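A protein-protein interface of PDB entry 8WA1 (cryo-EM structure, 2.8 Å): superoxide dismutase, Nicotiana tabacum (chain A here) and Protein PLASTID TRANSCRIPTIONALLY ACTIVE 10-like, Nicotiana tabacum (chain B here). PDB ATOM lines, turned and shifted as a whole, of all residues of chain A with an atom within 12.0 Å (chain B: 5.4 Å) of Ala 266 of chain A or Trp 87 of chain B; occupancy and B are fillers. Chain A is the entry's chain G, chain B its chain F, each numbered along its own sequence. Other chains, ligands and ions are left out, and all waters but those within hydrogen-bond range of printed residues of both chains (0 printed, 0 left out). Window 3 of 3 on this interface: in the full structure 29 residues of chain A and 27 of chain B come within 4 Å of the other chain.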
ATOM      1  N   PRO A 261      -2.463  27.154  -1.142  1.00  0.00           N
ATOM      2  CA  PRO A 261      -3.263  27.449   0.050  1.00  0.00           C
ATOM      3  C   PRO A 261      -3.795  26.178   0.693  1.00  0.00           C
ATOM      4  O   PRO A 261      -3.807  25.098   0.099  1.00  0.00           O
ATOM      5  CB  PRO A 261      -4.402  28.313  -0.496  1.00  0.00           C
ATOM      6  CG  PRO A 261      -4.561  27.850  -1.906  1.00  0.00           C
ATOM      7  CD  PRO A 261      -3.178  27.487  -2.386  1.00  0.00           C
ATOM      8  N   LYS A 262      -4.246  26.327   1.935  1.00  0.00           N
ATOM      9  CA  LYS A 262      -4.808  25.226   2.706  1.00  0.00           C
ATOM     10  C   LYS A 262      -6.303  25.147   2.428  1.00  0.00           C
ATOM     11  O   LYS A 262      -7.040  26.103   2.692  1.00  0.00           O
ATOM     12  CB  LYS A 262      -4.544  25.416   4.199  1.00  0.00           C
ATOM     13  CG  LYS A 262      -5.124  24.321   5.079  1.00  0.00           C
ATOM     14  CD  LYS A 262      -4.819  24.573   6.547  1.00  0.00           C
ATOM     15  CE  LYS A 262      -5.411  23.482   7.428  1.00  0.00           C
ATOM     16  NZ  LYS A 262      -5.117  23.706   8.871  1.00  0.00           N
ATOM     17  N   ILE A 263      -6.746  24.013   1.900  1.00  0.00           N
ATOM     18  CA  ILE A 263      -8.138  23.808   1.510  1.00  0.00           C
ATOM     19  C   ILE A 263      -8.838  23.055   2.636  1.00  0.00           C
ATOM     20  O   ILE A 263      -8.550  21.866   2.840  1.00  0.00           O
ATOM     21  CB  ILE A 263      -8.245  23.036   0.187  1.00  0.00           C
ATOM     22  CG1 ILE A 263      -7.269  23.602  -0.844  1.00  0.00           C
ATOM     23  CG2 ILE A 263      -9.667  23.088  -0.343  1.00  0.00           C
ATOM     24  CD1 ILE A 263      -7.501  25.055  -1.172  1.00  0.00           C
ATOM     25  N   PRO A 264      -9.744  23.688   3.379  1.00  0.00           N
ATOM     26  CA  PRO A 264     -10.457  22.968   4.439  1.00  0.00           C
ATOM     27  C   PRO A 264     -11.384  21.911   3.859  1.00  0.00           C
ATOM     28  O   PRO A 264     -12.061  22.135   2.854  1.00  0.00           O
ATOM     29  CB  PRO A 264     -11.243  24.073   5.155  1.00  0.00           C
ATOM     30  CG  PRO A 264     -10.595  25.357   4.730  1.00  0.00           C
ATOM     31  CD  PRO A 264     -10.098  25.114   3.345  1.00  0.00           C
ATOM     32  N   VAL A 265     -11.408  20.749   4.505  1.00  0.00           N
ATOM     33  CA  VAL A 265     -12.276  19.653   4.084  1.00  0.00           C
ATOM     34  C   VAL A 265     -13.675  19.925   4.628  1.00  0.00           C
ATOM     35  O   VAL A 265     -13.921  19.796   5.829  1.00  0.00           O
ATOM     36  CB  VAL A 265     -11.748  18.298   4.563  1.00  0.00           C
ATOM     37  CG1 VAL A 265     -12.660  17.180   4.087  1.00  0.00           C
ATOM     38  CG2 VAL A 265     -10.324  18.079   4.073  1.00  0.00           C
ATOM     39  N   ALA A 266     -14.594  20.298   3.744  1.00  0.00           N
ATOM     40  CA  ALA A 266     -15.962  20.608   4.141  1.00  0.00           C
ATOM     41  C   ALA A 266     -16.926  20.396   2.980  1.00  0.00           C
ATOM     42  O   ALA A 266     -17.802  21.224   2.729  1.00  0.00           O
ATOM     43  CB  ALA A 266     -16.054  22.035   4.655  1.00  0.00           C
ATOM     44  N   ARG B  78     -12.894  20.687  -5.178  1.00  0.00           N
ATOM     45  CA  ARG B  78     -12.931  21.663  -4.093  1.00  0.00           C
ATOM     46  C   ARG B  78     -11.727  22.594  -4.149  1.00  0.00           C
ATOM     47  O   ARG B  78     -11.853  23.801  -3.901  1.00  0.00           O
ATOM     48  CB  ARG B  78     -12.998  20.939  -2.748  1.00  0.00           C
ATOM     49  CG  ARG B  78     -12.946  21.855  -1.539  1.00  0.00           C
ATOM     50  CD  ARG B  78     -13.317  21.124  -0.255  1.00  0.00           C
ATOM     51  NE  ARG B  78     -12.481  19.951  -0.013  1.00  0.00           N
ATOM     52  CZ  ARG B  78     -12.879  18.697  -0.201  1.00  0.00           C
ATOM     53  NH1 ARG B  78     -14.108  18.446  -0.633  1.00  0.00           N
ATOM     54  NH2 ARG B  78     -12.050  17.691   0.047  1.00  0.00           N
ATOM     55  N   ASN B  81     -12.394  25.045  -6.916  1.00  0.00           N
ATOM     56  CA  ASN B  81     -13.359  26.042  -6.463  1.00  0.00           C
ATOM     57  C   ASN B  81     -12.693  27.086  -5.578  1.00  0.00           C
ATOM     58  O   ASN B  81     -12.859  28.291  -5.798  1.00  0.00           O
ATOM     59  CB  ASN B  81     -14.510  25.367  -5.715  1.00  0.00           C
ATOM     60  CG  ASN B  81     -15.418  24.571  -6.633  1.00  0.00           C
ATOM     61  OD1 ASN B  81     -15.710  23.404  -6.375  1.00  0.00           O
ATOM     62  ND2 ASN B  81     -15.871  25.201  -7.709  1.00  0.00           N
ATOM     63  N   TRP B  82     -11.913  26.641  -4.590  1.00  0.00           N
ATOM     64  CA  TRP B  82     -11.244  27.574  -3.687  1.00  0.00           C
ATOM     65  C   TRP B  82     -10.297  28.495  -4.448  1.00  0.00           C
ATOM     66  O   TRP B  82     -10.193  29.688  -4.140  1.00  0.00           O
ATOM     67  CB  TRP B  82     -10.488  26.801  -2.603  1.00  0.00           C
ATOM     68  CG  TRP B  82      -9.750  27.678  -1.626  1.00  0.00           C
ATOM     69  CD1 TRP B  82      -8.569  28.331  -1.838  1.00  0.00           C
ATOM     70  CD2 TRP B  82     -10.136  27.980  -0.278  1.00  0.00           C
ATOM     71  NE1 TRP B  82      -8.204  29.028  -0.712  1.00  0.00           N
ATOM     72  CE2 TRP B  82      -9.148  28.828   0.259  1.00  0.00           C
ATOM     73  CE3 TRP B  82     -11.223  27.618   0.523  1.00  0.00           C
ATOM     74  CZ2 TRP B  82      -9.214  29.321   1.561  1.00  0.00           C
ATOM     75  CZ3 TRP B  82     -11.287  28.110   1.814  1.00  0.00           C
ATOM     76  CH2 TRP B  82     -10.290  28.950   2.320  1.00  0.00           C
ATOM     77  N   ARG B  85     -13.038  30.154  -8.019  1.00  0.00           N
ATOM     78  CA  ARG B  85     -14.353  30.734  -7.789  1.00  0.00           C
ATOM     79  C   ARG B  85     -14.490  31.383  -6.418  1.00  0.00           C
ATOM     80  O   ARG B  85     -15.507  32.032  -6.156  1.00  0.00           O
ATOM     81  CB  ARG B  85     -15.433  29.663  -7.968  1.00  0.00           C
ATOM     82  CG  ARG B  85     -15.300  28.882  -9.264  1.00  0.00           C
ATOM     83  CD  ARG B  85     -16.465  27.932  -9.468  1.00  0.00           C
ATOM     84  NE  ARG B  85     -16.245  27.045 -10.607  1.00  0.00           N
ATOM     85  CZ  ARG B  85     -16.556  27.350 -11.862  1.00  0.00           C
ATOM     86  NH1 ARG B  85     -16.317  26.480 -12.835  1.00  0.00           N
ATOM     87  NH2 ARG B  85     -17.102  28.524 -12.147  1.00  0.00           N
ATOM     88  N   GLY B  86     -13.499  31.231  -5.545  1.00  0.00           N
ATOM     89  CA  GLY B  86     -13.542  31.883  -4.252  1.00  0.00           C
ATOM     90  C   GLY B  86     -14.387  31.193  -3.208  1.00  0.00           C
ATOM     91  O   GLY B  86     -14.922  31.864  -2.321  1.00  0.00           O
ATOM     92  N   TRP B  87     -14.530  29.873  -3.284  1.00  0.00           N
ATOM     93  CA  TRP B  87     -15.310  29.148  -2.292  1.00  0.00           C
ATOM     94  C   TRP B  87     -14.602  29.164  -0.942  1.00  0.00           C
ATOM     95  O   TRP B  87     -13.373  29.205  -0.859  1.00  0.00           O
ATOM     96  CB  TRP B  87     -15.545  27.708  -2.747  1.00  0.00           C
ATOM     97  CG  TRP B  87     -16.211  26.847  -1.717  1.00  0.00           C
ATOM     98  CD1 TRP B  87     -17.546  26.773  -1.449  1.00  0.00           C
ATOM     99  CD2 TRP B  87     -15.569  25.933  -0.819  1.00  0.00           C
ATOM    100  NE1 TRP B  87     -17.776  25.872  -0.438  1.00  0.00           N
ATOM    101  CE2 TRP B  87     -16.579  25.343  -0.033  1.00  0.00           C
ATOM    102  CE3 TRP B  87     -14.240  25.560  -0.602  1.00  0.00           C
ATOM    103  CZ2 TRP B  87     -16.300  24.398   0.952  1.00  0.00           C
ATOM    104  CZ3 TRP B  87     -13.967  24.623   0.377  1.00  0.00           C
ATOM    105  CH2 TRP B  87     -14.992  24.052   1.140  1.00  0.00           C
ATOM    106  N   ALA B  88     -15.398  29.145   0.124  1.00  0.00           N
ATOM    107  CA  ALA B  88     -14.881  29.106   1.484  1.00  0.00           C
ATOM    108  C   ALA B  88     -15.974  28.586   2.403  1.00  0.00           C
ATOM    109  O   ALA B  88     -17.144  28.956   2.241  1.00  0.00           O
ATOM    110  CB  ALA B  88     -14.408  30.490   1.953  1.00  0.00           C
ATOM    111  N   PRO B  89     -15.632  27.732   3.369  1.00  0.00           N
ATOM    112  CA  PRO B  89     -16.639  27.177   4.292  1.00  0.00           C
ATOM    113  C   PRO B  89     -17.038  28.171   5.379  1.00  0.00           C
ATOM    114  O   PRO B  89     -16.738  27.995   6.563  1.00  0.00           O
ATOM    115  CB  PRO B  89     -15.921  25.943   4.862  1.00  0.00           C
ATOM    116  CG  PRO B  89     -14.634  25.797   4.089  1.00  0.00           C
ATOM    117  CD  PRO B  89     -14.302  27.155   3.599  1.00  0.00           C
ATOM    118  N   ASN B 310     -11.058  35.518  -0.363  1.00  0.00           N
ATOM    119  CA  ASN B 310     -10.867  34.149   0.096  1.00  0.00           C
ATOM    120  C   ASN B 310      -9.773  33.987   1.138  1.00  0.00           C
ATOM    121  O   ASN B 310      -9.785  32.991   1.867  1.00  0.00           O
ATOM    122  CB  ASN B 310     -10.557  33.226  -1.091  1.00  0.00           C
ATOM    123  CG  ASN B 310     -11.456  32.007  -1.132  1.00  0.00           C
ATOM    124  OD1 ASN B 310     -12.529  31.995  -0.529  1.00  0.00           O
ATOM    125  ND2 ASN B 310     -11.024  30.976  -1.847  1.00  0.00           N
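The backbone carbonyl oxygen (O) of Asn 81 of chain B lies within hydrogen-bond range of the backbone NH (N) of Trp 87 of chain B (3.4 Å). The backbone carbonyl oxygen (O) of Trp 82 of chain B lies within hydrogen-bond range of the side-chain amide nitrogen (ND2) of Asn 310 of chain B (2.8 Å). The side-chain amide oxygen (OD1) of Asn 310 of chain B sits close to the backbone carbonyl oxygen (O) of Trp 87 of chain B, at 2.9 Å.
Pro 261 of chain A touches Trp 82 of chain B (CB to NE1, 3.9 Å). CG of Arg 78 of chain B touches CG2 of Ile 263 of chain A, at 3.7 Å. Trp 82 of chain B touches Ile 263 of chain A (CG to CD1, 3.5 Å). Pro 264 of chain A touches Arg 78 of chain B (O to CD, 3.5 Å). Pro 264 of chain A touches Trp 82 of chain B. Pro 264 of chain A touches Trp 87 of chain B. Pro 89 of chain B touches Pro 264 of chain A. Ala 266 of chain A touches Trp 87 of chain B. Ala 266 of chain A touches Pro 89 of chain B (CB to CB, 3.9 Å).
Of chain B, only Trp 87 (3.9 Å) and Pro 89 (3.9 Å) come within 4 Å of Ala 266 of chain A. Of chain A, only Pro 264 and Ala 266 come within 4 Å of Trp 87 of chain B. Of chain A, only Pro 261, Ile 263 and Pro 264 come within 4 Å of Trp 82 of chain B. Of chain A, only Pro 264 (3.95 Å) and Ala 266 (3.9 Å) come within 4 Å of Pro 89 of chain B. Of the printed residues of chain B, Pro 264 of chain A touches Arg 78, Trp 82, Trp 87 and Pro 89. Printed residues of chain B within 4 Å of Ile 263 of chain A: Arg 78 (3.7 Å) and Trp 82 (3.5 Å). Printed residues of chain B within 4 Å of Pro 261 of chain A: Trp 82. Val 265 of chain A touches none of the printed residues of chain B. The nearest residue of chain B that does not touch Ala 266 of chain A is Arg 78 of chain B (4.3 Å). The nearest residue of chain A that does not touch Trp 87 of chain B is Ile 263 of chain A (4.6 Å).
Of the 9 printed residues of chain B, 4 touch a printed residue of chain A. Hydrophobic or aromatic side chains of chain B that line the printed part of chain A: Trp 82, Trp 87 and Pro 89.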
